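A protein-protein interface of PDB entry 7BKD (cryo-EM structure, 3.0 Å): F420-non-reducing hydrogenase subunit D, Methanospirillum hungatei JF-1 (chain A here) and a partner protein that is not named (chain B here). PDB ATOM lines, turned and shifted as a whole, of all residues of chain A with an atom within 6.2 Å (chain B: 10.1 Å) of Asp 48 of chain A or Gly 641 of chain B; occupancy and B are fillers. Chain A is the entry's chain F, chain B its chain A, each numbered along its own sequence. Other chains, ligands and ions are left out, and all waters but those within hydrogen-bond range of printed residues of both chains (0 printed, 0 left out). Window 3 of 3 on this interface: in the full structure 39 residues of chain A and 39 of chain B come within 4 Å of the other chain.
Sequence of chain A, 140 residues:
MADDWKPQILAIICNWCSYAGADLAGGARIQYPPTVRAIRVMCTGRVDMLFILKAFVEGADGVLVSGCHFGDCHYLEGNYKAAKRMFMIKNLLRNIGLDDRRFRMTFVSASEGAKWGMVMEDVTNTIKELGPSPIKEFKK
The side-chain sulfur (SD) of Met 650 of chain B sits close to the backbone NH (N) of Gly 640 of chain B. O of Gly 45 of chain A lies within hydrogen-bond range of NH1 of Arg 85 of chain A, 2.6 Å away. O of Val 47 of chain A sits at hydrogen-bond distance from NH1 of Arg 85 of chain A (3.1 Å). SG of Cys 636 of chain B sits close to N of Thr 638 of chain B (3.1 Å).
Of the printed residues of chain B, Gly 45 of chain A touches Gly 637 (3.6 Å) and Thr 638 (3.6 Å). Asp 48 of chain A touches one residue of chain B. No residue of chain B comes within 4 Å of Leu 50 of chain A. Phe 51 of chain A touches just these residues of chain B: Thr 655 (3.8 Å) and Ile 658 (3.9 Å). Printed residues of chain A within 4 Å of Gly 641 of chain B: Arg 46 and Asp 48. Of the printed residues of chain A, Phe 642 of chain B touches Arg 85. Gly 645 of chain B touches none of the printed residues of chain A. Of the printed residues of chain A, Met 650 of chain B touches Arg 46 (3.5 Å). The nearest residue of chain B that does not touch Asp 48 of chain A is Phe 642 of chain B (4.8 Å). The nearest residue of chain A that does not touch Gly 641 of chain B is Arg 85 of chain A (4.2 Å).
Among the printed residues, merely in contact across the chains: Arg 46 of chain A with Thr 654 of chain B, Arg 46 of chain A with Gly 637 of chain B, Arg 46 of chain A with Met 650 of chain B, Arg 46 of chain A with Gly 641 of chain B, Gly 45 of chain A with Gly 637 of chain B, Gly 45 of chain A with Thr 638 of chain B, Arg 85 of chain A with Phe 642 of chain B, Phe 51 of chain A with Thr 655 of chain B, Phe 51 of chain A with Ile 658 of chain B and Arg 46 of chain A with Gly 640 of chain B.
The guanidinium group of Arg 85 of chain A is in hydrogen-bond range of the backbone carbonyl oxygen of Thr 638 of chain B (3.3 Å). The backbone carbonyl oxygen of Phe 653 of chain B lies within hydrogen-bond range of the guanidinium group of Arg 46 of chain A, 2.8 Å away. The side-chain carboxylate of Asp 48 of chain A sits close to the backbone carbonyl oxygen of Gly 641 of chain B, 3.0 Å away. The side-chain hydroxyl (OG1) of Thr 655 of chain B lies within hydrogen-bond range of the guanidinium group (NH2) of Arg 46 of chain A, 3.2 Å away.
Of the 29 printed residues of chain B, 10 touch a printed residue of chain A. Hydrophobic or aromatic side chains of chain A within 4 Å of the printed part of chain B: Phe 51.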
ATOM      1  N   THR A  44      14.247 -34.929 -10.091  1.00  0.00           N
ATOM      2  CA  THR A  44      14.137 -33.645  -9.386  1.00  0.00           C
ATOM      3  C   THR A  44      15.279 -32.722  -9.804  1.00  0.00           C
ATOM      4  O   THR A  44      15.292 -31.542  -9.445  1.00  0.00           O
ATOM      5  CB  THR A  44      14.070 -33.758  -7.845  1.00  0.00           C
ATOM      6  OG1 THR A  44      13.773 -32.467  -7.310  1.00  0.00           O
ATOM      7  CG2 THR A  44      15.382 -34.111  -7.213  1.00  0.00           C
ATOM      8  N   GLY A  45      16.229 -33.244 -10.581  1.00  0.00           N
ATOM      9  CA  GLY A  45      17.094 -32.407 -11.384  1.00  0.00           C
ATOM     10  C   GLY A  45      16.469 -32.031 -12.701  1.00  0.00           C
ATOM     11  O   GLY A  45      16.946 -31.111 -13.367  1.00  0.00           O
ATOM     12  N   ARG A  46      15.407 -32.737 -13.086  1.00  0.00           N
ATOM     13  CA  ARG A  46      14.549 -32.304 -14.175  1.00  0.00           C
ATOM     14  C   ARG A  46      13.856 -30.992 -13.852  1.00  0.00           C
ATOM     15  O   ARG A  46      13.454 -30.271 -14.770  1.00  0.00           O
ATOM     16  CB  ARG A  46      13.517 -33.394 -14.469  1.00  0.00           C
ATOM     17  CG  ARG A  46      12.551 -33.094 -15.598  1.00  0.00           C
ATOM     18  CD  ARG A  46      13.269 -32.922 -16.916  1.00  0.00           C
ATOM     19  NE  ARG A  46      12.347 -32.534 -17.972  1.00  0.00           N
ATOM     20  CZ  ARG A  46      12.046 -31.277 -18.269  1.00  0.00           C
ATOM     21  NH1 ARG A  46      12.599 -30.285 -17.593  1.00  0.00           N
ATOM     22  NH2 ARG A  46      11.194 -31.013 -19.244  1.00  0.00           N
ATOM     23  N   VAL A  47      13.723 -30.660 -12.572  1.00  0.00           N
ATOM     24  CA  VAL A  47      12.974 -29.478 -12.160  1.00  0.00           C
ATOM     25  C   VAL A  47      13.725 -28.237 -12.628  1.00  0.00           C
ATOM     26  O   VAL A  47      14.797 -27.912 -12.112  1.00  0.00           O
ATOM     27  CB  VAL A  47      12.754 -29.453 -10.646  1.00  0.00           C
ATOM     28  CG1 VAL A  47      11.829 -28.320 -10.274  1.00  0.00           C
ATOM     29  CG2 VAL A  47      12.181 -30.760 -10.193  1.00  0.00           C
ATOM     30  N   ASP A  48      13.165 -27.554 -13.617  1.00  0.00           N
ATOM     31  CA  ASP A  48      13.635 -26.241 -14.011  1.00  0.00           C
ATOM     32  C   ASP A  48      13.095 -25.192 -13.045  1.00  0.00           C
ATOM     33  O   ASP A  48      12.087 -25.398 -12.367  1.00  0.00           O
ATOM     34  CB  ASP A  48      13.190 -25.924 -15.439  1.00  0.00           C
ATOM     35  CG  ASP A  48      13.915 -24.731 -16.028  1.00  0.00           C
ATOM     36  OD1 ASP A  48      14.764 -24.140 -15.328  1.00  0.00           O
ATOM     37  OD2 ASP A  48      13.636 -24.384 -17.195  1.00  0.00           O
ATOM     38  N   MET A  49      13.790 -24.057 -12.978  1.00  0.00           N
ATOM     39  CA  MET A  49      13.275 -22.941 -12.194  1.00  0.00           C
ATOM     40  C   MET A  49      11.958 -22.439 -12.750  1.00  0.00           C
ATOM     41  O   MET A  49      11.093 -21.984 -11.992  1.00  0.00           O
ATOM     42  CB  MET A  49      14.282 -21.803 -12.164  1.00  0.00           C
ATOM     43  CG  MET A  49      15.531 -22.124 -11.414  1.00  0.00           C
ATOM     44  SD  MET A  49      16.652 -20.735 -11.438  1.00  0.00           S
ATOM     45  CE  MET A  49      18.010 -21.472 -10.573  1.00  0.00           C
ATOM     46  N   LEU A  50      11.794 -22.508 -14.068  1.00  0.00           N
ATOM     47  CA  LEU A  50      10.577 -22.005 -14.682  1.00  0.00           C
ATOM     48  C   LEU A  50       9.361 -22.806 -14.246  1.00  0.00           C
ATOM     49  O   LEU A  50       8.260 -22.261 -14.196  1.00  0.00           O
ATOM     50  CB  LEU A  50      10.729 -22.003 -16.201  1.00  0.00           C
ATOM     51  CG  LEU A  50      11.925 -21.193 -16.709  1.00  0.00           C
ATOM     52  CD1 LEU A  50      11.862 -20.999 -18.204  1.00  0.00           C
ATOM     53  CD2 LEU A  50      12.000 -19.853 -16.010  1.00  0.00           C
ATOM     54  N   PHE A  51       9.539 -24.079 -13.886  1.00  0.00           N
ATOM     55  CA  PHE A  51       8.432 -24.849 -13.324  1.00  0.00           C
ATOM     56  C   PHE A  51       7.937 -24.228 -12.023  1.00  0.00           C
ATOM     57  O   PHE A  51       6.736 -23.993 -11.846  1.00  0.00           O
ATOM     58  CB  PHE A  51       8.860 -26.296 -13.080  1.00  0.00           C
ATOM     59  CG  PHE A  51       9.208 -27.051 -14.324  1.00  0.00           C
ATOM     60  CD1 PHE A  51       8.807 -26.600 -15.564  1.00  0.00           C
ATOM     61  CD2 PHE A  51       9.937 -28.222 -14.249  1.00  0.00           C
ATOM     62  CE1 PHE A  51       9.131 -27.298 -16.703  1.00  0.00           C
ATOM     63  CE2 PHE A  51      10.265 -28.921 -15.387  1.00  0.00           C
ATOM     64  CZ  PHE A  51       9.860 -28.458 -16.614  1.00  0.00           C
ATOM     65  N   ILE A  52       8.859 -23.953 -11.099  1.00  0.00           N
ATOM     66  CA  ILE A  52       8.487 -23.388  -9.805  1.00  0.00           C
ATOM     67  C   ILE A  52       7.890 -22.001  -9.982  1.00  0.00           C
ATOM     68  O   ILE A  52       6.883 -21.651  -9.351  1.00  0.00           O
ATOM     69  CB  ILE A  52       9.710 -23.358  -8.874  1.00  0.00           C
ATOM     70  CG1 ILE A  52      10.419 -24.710  -8.885  1.00  0.00           C
ATOM     71  CG2 ILE A  52       9.296 -22.990  -7.470  1.00  0.00           C
ATOM     72  CD1 ILE A  52       9.675 -25.792  -8.159  1.00  0.00           C
ATOM     73  N   LEU A  53       8.502 -21.186 -10.841  1.00  0.00           N
ATOM     74  CA  LEU A  53       8.004 -19.832 -11.048  1.00  0.00           C
ATOM     75  C   LEU A  53       6.638 -19.834 -11.722  1.00  0.00           C
ATOM     76  O   LEU A  53       5.774 -19.022 -11.382  1.00  0.00           O
ATOM     77  CB  LEU A  53       9.017 -19.029 -11.857  1.00  0.00           C
ATOM     78  CG  LEU A  53      10.337 -18.846 -11.113  1.00  0.00           C
ATOM     79  CD1 LEU A  53      11.405 -18.311 -12.034  1.00  0.00           C
ATOM     80  CD2 LEU A  53      10.140 -17.927  -9.931  1.00  0.00           C
ATOM     81  N   ARG A  85      19.602 -24.896  -7.736  1.00  0.00           N
ATOM     82  CA  ARG A  85      18.475 -24.193  -8.330  1.00  0.00           C
ATOM     83  C   ARG A  85      17.495 -23.723  -7.268  1.00  0.00           C
ATOM     84  O   ARG A  85      16.959 -22.617  -7.361  1.00  0.00           O
ATOM     85  CB  ARG A  85      17.788 -25.087  -9.356  1.00  0.00           C
ATOM     86  CG  ARG A  85      18.562 -25.192 -10.643  1.00  0.00           C
ATOM     87  CD  ARG A  85      17.926 -26.160 -11.600  1.00  0.00           C
ATOM     88  NE  ARG A  85      18.929 -26.800 -12.439  1.00  0.00           N
ATOM     89  CZ  ARG A  85      18.811 -28.023 -12.936  1.00  0.00           C
ATOM     90  NH1 ARG A  85      17.730 -28.736 -12.677  1.00  0.00           N
ATOM     91  NH2 ARG A  85      19.772 -28.530 -13.689  1.00  0.00           N
ATOM     92  N   MET A  86      17.265 -24.532  -6.238  1.00  0.00           N
ATOM     93  CA  MET A  86      16.291 -24.150  -5.226  1.00  0.00           C
ATOM     94  C   MET A  86      16.838 -23.093  -4.277  1.00  0.00           C
ATOM     95  O   MET A  86      16.072 -22.256  -3.788  1.00  0.00           O
ATOM     96  CB  MET A  86      15.816 -25.378  -4.454  1.00  0.00           C
ATOM     97  CG  MET A  86      15.275 -26.486  -5.351  1.00  0.00           C
ATOM     98  SD  MET A  86      13.926 -26.019  -6.449  1.00  0.00           S
ATOM     99  CE  MET A  86      14.539 -26.609  -8.020  1.00  0.00           C
ATOM    100  N   ALA B 593      17.495 -37.965 -23.727  1.00  0.00           N
ATOM    101  CA  ALA B 593      17.393 -36.558 -24.145  1.00  0.00           C
ATOM    102  C   ALA B 593      17.680 -36.436 -25.627  1.00  0.00           C
ATOM    103  O   ALA B 593      18.545 -37.161 -26.115  1.00  0.00           O
ATOM    104  CB  ALA B 593      18.405 -35.761 -23.414  1.00  0.00           C
ATOM    105  N   MET B 594      16.981 -35.536 -26.304  1.00  0.00           N
ATOM    106  CA  MET B 594      17.240 -35.255 -27.726  1.00  0.00           C
ATOM    107  C   MET B 594      17.583 -33.775 -27.816  1.00  0.00           C
ATOM    108  O   MET B 594      16.920 -32.997 -27.151  1.00  0.00           O
ATOM    109  CB  MET B 594      15.967 -35.505 -28.532  1.00  0.00           C
ATOM    110  CG  MET B 594      15.195 -36.723 -28.104  1.00  0.00           C
ATOM    111  SD  MET B 594      13.668 -36.855 -29.049  1.00  0.00           S
ATOM    112  CE  MET B 594      14.053 -38.251 -30.104  1.00  0.00           C
ATOM    113  N   CYS B 606      25.823 -27.075 -20.657  1.00  0.00           N
ATOM    114  CA  CYS B 606      25.258 -28.353 -20.252  1.00  0.00           C
ATOM    115  C   CYS B 606      26.245 -29.502 -20.344  1.00  0.00           C
ATOM    116  O   CYS B 606      25.984 -30.558 -19.767  1.00  0.00           O
ATOM    117  CB  CYS B 606      24.039 -28.671 -21.112  1.00  0.00           C
ATOM    118  SG  CYS B 606      24.384 -28.687 -22.880  1.00  0.00           S
ATOM    119  N   LEU B 609      27.488 -30.903 -17.187  1.00  0.00           N
ATOM    120  CA  LEU B 609      26.384 -31.027 -16.255  1.00  0.00           C
ATOM    121  C   LEU B 609      25.824 -32.436 -16.176  1.00  0.00           C
ATOM    122  O   LEU B 609      25.019 -32.712 -15.283  1.00  0.00           O
ATOM    123  CB  LEU B 609      25.269 -30.053 -16.650  1.00  0.00           C
ATOM    124  CG  LEU B 609      24.374 -29.509 -15.553  1.00  0.00           C
ATOM    125  CD1 LEU B 609      25.163 -28.523 -14.732  1.00  0.00           C
ATOM    126  CD2 LEU B 609      23.177 -28.840 -16.170  1.00  0.00           C
ATOM    127  N   LEU B 615      26.861 -35.741 -23.033  1.00  0.00           N
ATOM    128  CA  LEU B 615      26.663 -34.532 -23.813  1.00  0.00           C
ATOM    129  C   LEU B 615      28.011 -34.031 -24.310  1.00  0.00           C
ATOM    130  O   LEU B 615      28.969 -33.956 -23.537  1.00  0.00           O
ATOM    131  CB  LEU B 615      25.998 -33.459 -22.960  1.00  0.00           C
ATOM    132  CG  LEU B 615      24.579 -33.753 -22.477  1.00  0.00           C
ATOM    133  CD1 LEU B 615      24.103 -32.662 -21.545  1.00  0.00           C
ATOM    134  CD2 LEU B 615      23.595 -34.019 -23.571  1.00  0.00           C
ATOM    135  N   GLY B 635      18.134 -40.594 -19.022  1.00  0.00           N
ATOM    136  CA  GLY B 635      16.849 -39.997 -18.740  1.00  0.00           C
ATOM    137  C   GLY B 635      16.755 -39.306 -17.407  1.00  0.00           C
ATOM    138  O   GLY B 635      15.655 -39.154 -16.878  1.00  0.00           O
ATOM    139  N   CYS B 636      17.883 -38.885 -16.839  1.00  0.00           N
ATOM    140  CA  CYS B 636      17.842 -38.176 -15.567  1.00  0.00           C
ATOM    141  C   CYS B 636      17.090 -36.861 -15.697  1.00  0.00           C
ATOM    142  O   CYS B 636      16.266 -36.523 -14.842  1.00  0.00           O
ATOM    143  CB  CYS B 636      19.258 -37.942 -15.053  1.00  0.00           C
ATOM    144  SG  CYS B 636      20.065 -36.493 -15.713  1.00  0.00           S
ATOM    145  N   GLY B 637      17.346 -36.117 -16.767  1.00  0.00           N
ATOM    146  CA  GLY B 637      16.671 -34.865 -17.014  1.00  0.00           C
ATOM    147  C   GLY B 637      17.406 -33.631 -16.553  1.00  0.00           C
ATOM    148  O   GLY B 637      16.841 -32.537 -16.631  1.00  0.00           O
ATOM    149  N   THR B 638      18.640 -33.768 -16.072  1.00  0.00           N
ATOM    150  CA  THR B 638      19.359 -32.619 -15.536  1.00  0.00           C
ATOM    151  C   THR B 638      19.596 -31.568 -16.609  1.00  0.00           C
ATOM    152  O   THR B 638      19.383 -30.374 -16.383  1.00  0.00           O
ATOM    153  CB  THR B 638      20.686 -33.068 -14.931  1.00  0.00           C
ATOM    154  OG1 THR B 638      20.436 -33.965 -13.844  1.00  0.00           O
ATOM    155  CG2 THR B 638      21.467 -31.884 -14.422  1.00  0.00           C
ATOM    156  N   CYS B 639      20.037 -31.999 -17.789  1.00  0.00           N
ATOM    157  CA  CYS B 639      20.317 -31.059 -18.867  1.00  0.00           C
ATOM    158  C   CYS B 639      19.050 -30.365 -19.337  1.00  0.00           C
ATOM    159  O   CYS B 639      19.039 -29.147 -19.532  1.00  0.00           O
ATOM    160  CB  CYS B 639      20.979 -31.790 -20.028  1.00  0.00           C
ATOM    161  SG  CYS B 639      20.073 -33.243 -20.581  1.00  0.00           S
ATOM    162  N   GLY B 640      17.972 -31.122 -19.524  1.00  0.00           N
ATOM    163  CA  GLY B 640      16.741 -30.531 -20.009  1.00  0.00           C
ATOM    164  C   GLY B 640      16.168 -29.506 -19.060  1.00  0.00           C
ATOM    165  O   GLY B 640      15.557 -28.528 -19.493  1.00  0.00           O
ATOM    166  N   GLY B 641      16.347 -29.711 -17.763  1.00  0.00           N
ATOM    167  CA  GLY B 641      15.880 -28.742 -16.799  1.00  0.00           C
ATOM    168  C   GLY B 641      16.743 -27.513 -16.661  1.00  0.00           C
ATOM    169  O   GLY B 641      16.324 -26.551 -16.014  1.00  0.00           O
ATOM    170  N   PHE B 642      17.933 -27.511 -17.251  1.00  0.00           N
ATOM    171  CA  PHE B 642      18.831 -26.375 -17.124  1.00  0.00           C
ATOM    172  C   PHE B 642      18.796 -25.447 -18.328  1.00  0.00           C
ATOM    173  O   PHE B 642      18.627 -24.238 -18.158  1.00  0.00           O
ATOM    174  CB  PHE B 642      20.266 -26.844 -16.902  1.00  0.00           C
ATOM    175  CG  PHE B 642      21.283 -25.821 -17.280  1.00  0.00           C
ATOM    176  CD1 PHE B 642      21.407 -24.653 -16.554  1.00  0.00           C
ATOM    177  CD2 PHE B 642      22.102 -26.010 -18.370  1.00  0.00           C
ATOM    178  CE1 PHE B 642      22.329 -23.706 -16.904  1.00  0.00           C
ATOM    179  CE2 PHE B 642      23.028 -25.062 -18.720  1.00  0.00           C
ATOM    180  CZ  PHE B 642      23.140 -23.912 -17.984  1.00  0.00           C
ATOM    181  N   CYS B 643      18.975 -25.989 -19.537  1.00  0.00           N
ATOM    182  CA  CYS B 643      19.121 -25.219 -20.768  1.00  0.00           C
ATOM    183  C   CYS B 643      18.101 -24.094 -20.830  1.00  0.00           C
ATOM    184  O   CYS B 643      16.891 -24.350 -20.841  1.00  0.00           O
ATOM    185  CB  CYS B 643      18.976 -26.119 -21.994  1.00  0.00           C
ATOM    186  SG  CYS B 643      19.210 -25.273 -23.572  1.00  0.00           S
ATOM    187  N   PRO B 644      18.550 -22.841 -20.831  1.00  0.00           N
ATOM    188  CA  PRO B 644      17.590 -21.733 -20.861  1.00  0.00           C
ATOM    189  C   PRO B 644      16.745 -21.717 -22.115  1.00  0.00           C
ATOM    190  O   PRO B 644      15.554 -21.395 -22.054  1.00  0.00           O
ATOM    191  CB  PRO B 644      18.489 -20.496 -20.760  1.00  0.00           C
ATOM    192  CG  PRO B 644      19.824 -21.000 -20.339  1.00  0.00           C
ATOM    193  CD  PRO B 644      19.938 -22.366 -20.879  1.00  0.00           C
ATOM    194  N   GLY B 645      17.321 -22.080 -23.251  1.00  0.00           N
ATOM    195  CA  GLY B 645      16.622 -21.981 -24.506  1.00  0.00           C
ATOM    196  C   GLY B 645      15.631 -23.073 -24.788  1.00  0.00           C
ATOM    197  O   GLY B 645      14.925 -23.003 -25.795  1.00  0.00           O
ATOM    198  N   GLY B 646      15.543 -24.082 -23.929  1.00  0.00           N
ATOM    199  CA  GLY B 646      14.636 -25.184 -24.184  1.00  0.00           C
ATOM    200  C   GLY B 646      15.005 -25.984 -25.412  1.00  0.00           C
ATOM    201  O   GLY B 646      14.120 -26.437 -26.146  1.00  0.00           O
ATOM    202  N   ALA B 647      16.297 -26.167 -25.653  1.00  0.00           N
ATOM    203  CA  ALA B 647      16.780 -26.888 -26.818  1.00  0.00           C
ATOM    204  C   ALA B 647      17.024 -28.363 -26.551  1.00  0.00           C
ATOM    205  O   ALA B 647      17.488 -29.068 -27.449  1.00  0.00           O
ATOM    206  CB  ALA B 647      18.067 -26.250 -27.334  1.00  0.00           C
ATOM    207  N   ILE B 648      16.738 -28.846 -25.347  1.00  0.00           N
ATOM    208  CA  ILE B 648      16.911 -30.248 -24.999  1.00  0.00           C
ATOM    209  C   ILE B 648      15.541 -30.828 -24.699  1.00  0.00           C
ATOM    210  O   ILE B 648      14.791 -30.271 -23.891  1.00  0.00           O
ATOM    211  CB  ILE B 648      17.853 -30.430 -23.800  1.00  0.00           C
ATOM    212  CG1 ILE B 648      19.283 -30.096 -24.201  1.00  0.00           C
ATOM    213  CG2 ILE B 648      17.797 -31.847 -23.313  1.00  0.00           C
ATOM    214  CD1 ILE B 648      20.204 -29.895 -23.040  1.00  0.00           C
ATOM    215  N   LYS B 649      15.215 -31.939 -25.349  1.00  0.00           N
ATOM    216  CA  LYS B 649      13.894 -32.542 -25.266  1.00  0.00           C
ATOM    217  C   LYS B 649      13.984 -33.828 -24.453  1.00  0.00           C
ATOM    218  O   LYS B 649      14.516 -34.834 -24.928  1.00  0.00           O
ATOM    219  CB  LYS B 649      13.348 -32.802 -26.667  1.00  0.00           C
ATOM    220  CG  LYS B 649      11.951 -33.371 -26.716  1.00  0.00           C
ATOM    221  CD  LYS B 649      11.481 -33.478 -28.146  1.00  0.00           C
ATOM    222  CE  LYS B 649      10.146 -34.180 -28.242  1.00  0.00           C
ATOM    223  NZ  LYS B 649       9.067 -33.383 -27.604  1.00  0.00           N
ATOM    224  N   MET B 650      13.474 -33.787 -23.225  1.00  0.00           N
ATOM    225  CA  MET B 650      13.355 -34.963 -22.364  1.00  0.00           C
ATOM    226  C   MET B 650      12.040 -35.640 -22.702  1.00  0.00           C
ATOM    227  O   MET B 650      10.990 -35.279 -22.181  1.00  0.00           O
ATOM    228  CB  MET B 650      13.395 -34.564 -20.893  1.00  0.00           C
ATOM    229  CG  MET B 650      14.476 -33.579 -20.491  1.00  0.00           C
ATOM    230  SD  MET B 650      16.145 -34.011 -20.993  1.00  0.00           S
ATOM    231  CE  MET B 650      16.179 -35.761 -20.614  1.00  0.00           C
ATOM    232  N   GLN B 651      12.087 -36.640 -23.574  1.00  0.00           N
ATOM    233  CA  GLN B 651      10.850 -37.227 -24.067  1.00  0.00           C
ATOM    234  C   GLN B 651      10.099 -37.947 -22.955  1.00  0.00           C
ATOM    235  O   GLN B 651      10.701 -38.542 -22.058  1.00  0.00           O
ATOM    236  CB  GLN B 651      11.127 -38.179 -25.225  1.00  0.00           C
ATOM    237  CG  GLN B 651      12.373 -38.995 -25.084  1.00  0.00           C
ATOM    238  CD  GLN B 651      12.686 -39.753 -26.345  1.00  0.00           C
ATOM    239  OE1 GLN B 651      11.917 -39.726 -27.301  1.00  0.00           O
ATOM    240  NE2 GLN B 651      13.810 -40.443 -26.355  1.00  0.00           N
ATOM    241  N   PHE B 653       8.788 -36.608 -20.653  1.00  0.00           N
ATOM    242  CA  PHE B 653       8.863 -35.650 -19.558  1.00  0.00           C
ATOM    243  C   PHE B 653       9.249 -34.288 -20.099  1.00  0.00           C
ATOM    244  O   PHE B 653      10.062 -33.573 -19.509  1.00  0.00           O
ATOM    245  CB  PHE B 653       9.850 -36.107 -18.488  1.00  0.00           C
ATOM    246  CG  PHE B 653       9.337 -37.225 -17.633  1.00  0.00           C
ATOM    247  CD1 PHE B 653       8.486 -36.970 -16.579  1.00  0.00           C
ATOM    248  CD2 PHE B 653       9.700 -38.531 -17.890  1.00  0.00           C
ATOM    249  CE1 PHE B 653       8.011 -37.993 -15.799  1.00  0.00           C
ATOM    250  CE2 PHE B 653       9.226 -39.555 -17.111  1.00  0.00           C
ATOM    251  CZ  PHE B 653       8.381 -39.285 -16.066  1.00  0.00           C
ATOM    252  N   THR B 654       8.689 -33.923 -21.247  1.00  0.00           N
ATOM    253  CA  THR B 654       9.056 -32.680 -21.898  1.00  0.00           C
ATOM    254  C   THR B 654       8.483 -31.492 -21.140  1.00  0.00           C
ATOM    255  O   THR B 654       7.510 -31.606 -20.392  1.00  0.00           O
ATOM    256  CB  THR B 654       8.553 -32.648 -23.339  1.00  0.00           C
ATOM    257  OG1 THR B 654       7.207 -33.121 -23.383  1.00  0.00           O
ATOM    258  CG2 THR B 654       9.402 -33.531 -24.211  1.00  0.00           C
ATOM    259  N   THR B 655       9.111 -30.337 -21.340  1.00  0.00           N
ATOM    260  CA  THR B 655       8.608 -29.103 -20.743  1.00  0.00           C
ATOM    261  C   THR B 655       7.144 -28.842 -21.070  1.00  0.00           C
ATOM    262  O   THR B 655       6.388 -28.507 -20.148  1.00  0.00           O
ATOM    263  CB  THR B 655       9.499 -27.929 -21.170  1.00  0.00           C
ATOM    264  OG1 THR B 655      10.857 -28.203 -20.812  1.00  0.00           O
ATOM    265  CG2 THR B 655       9.061 -26.658 -20.486  1.00  0.00           C
ATOM    266  N   PRO B 656       6.670 -28.984 -22.313  1.00  0.00           N
ATOM    267  CA  PRO B 656       5.233 -28.797 -22.552  1.00  0.00           C
ATOM    268  C   PRO B 656       4.338 -29.738 -21.762  1.00  0.00           C
ATOM    269  O   PRO B 656       3.247 -29.325 -21.356  1.00  0.00           O
ATOM    270  CB  PRO B 656       5.101 -29.029 -24.060  1.00  0.00           C
ATOM    271  CG  PRO B 656       6.408 -28.672 -24.595  1.00  0.00           C
ATOM    272  CD  PRO B 656       7.405 -29.108 -23.584  1.00  0.00           C
ATOM    273  N   ILE B 658       5.000 -31.250 -18.739  1.00  0.00           N
ATOM    274  CA  ILE B 658       5.026 -30.949 -17.311  1.00  0.00           C
ATOM    275  C   ILE B 658       4.264 -29.664 -17.022  1.00  0.00           C
ATOM    276  O   ILE B 658       3.505 -29.584 -16.052  1.00  0.00           O
ATOM    277  CB  ILE B 658       6.471 -30.879 -16.795  1.00  0.00           C
ATOM    278  CG1 ILE B 658       7.128 -32.251 -16.875  1.00  0.00           C
ATOM    279  CG2 ILE B 658       6.493 -30.396 -15.369  1.00  0.00           C
ATOM    280  CD1 ILE B 658       8.561 -32.254 -16.447  1.00  0.00           C
ATOM    281  N   VAL B 659       4.452 -28.639 -17.855  1.00  0.00           N
ATOM    282  CA  VAL B 659       3.690 -27.406 -17.688  1.00  0.00           C
ATOM    283  C   VAL B 659       2.205 -27.663 -17.877  1.00  0.00           C
ATOM    284  O   VAL B 659       1.369 -27.017 -17.235  1.00  0.00           O
ATOM    285  CB  VAL B 659       4.207 -26.320 -18.648  1.00  0.00           C
ATOM    286  CG1 VAL B 659       3.460 -25.027 -18.427  1.00  0.00           C
ATOM    287  CG2 VAL B 659       5.679 -26.082 -18.415  1.00  0.00           C
ATOM    288  N   ILE B 662       0.988 -28.777 -14.574  1.00  0.00           N
ATOM    289  CA  ILE B 662       0.913 -27.655 -13.646  1.00  0.00           C
ATOM    290  C   ILE B 662      -0.259 -26.752 -13.998  1.00  0.00           C
ATOM    291  O   ILE B 662      -0.944 -26.227 -13.114  1.00  0.00           O
ATOM    292  CB  ILE B 662       2.245 -26.883 -13.640  1.00  0.00           C
ATOM    293  CG1 ILE B 662       3.365 -27.758 -13.089  1.00  0.00           C
ATOM    294  CG2 ILE B 662       2.130 -25.623 -12.816  1.00  0.00           C
ATOM    295  CD1 ILE B 662       4.734 -27.192 -13.322  1.00  0.00           C
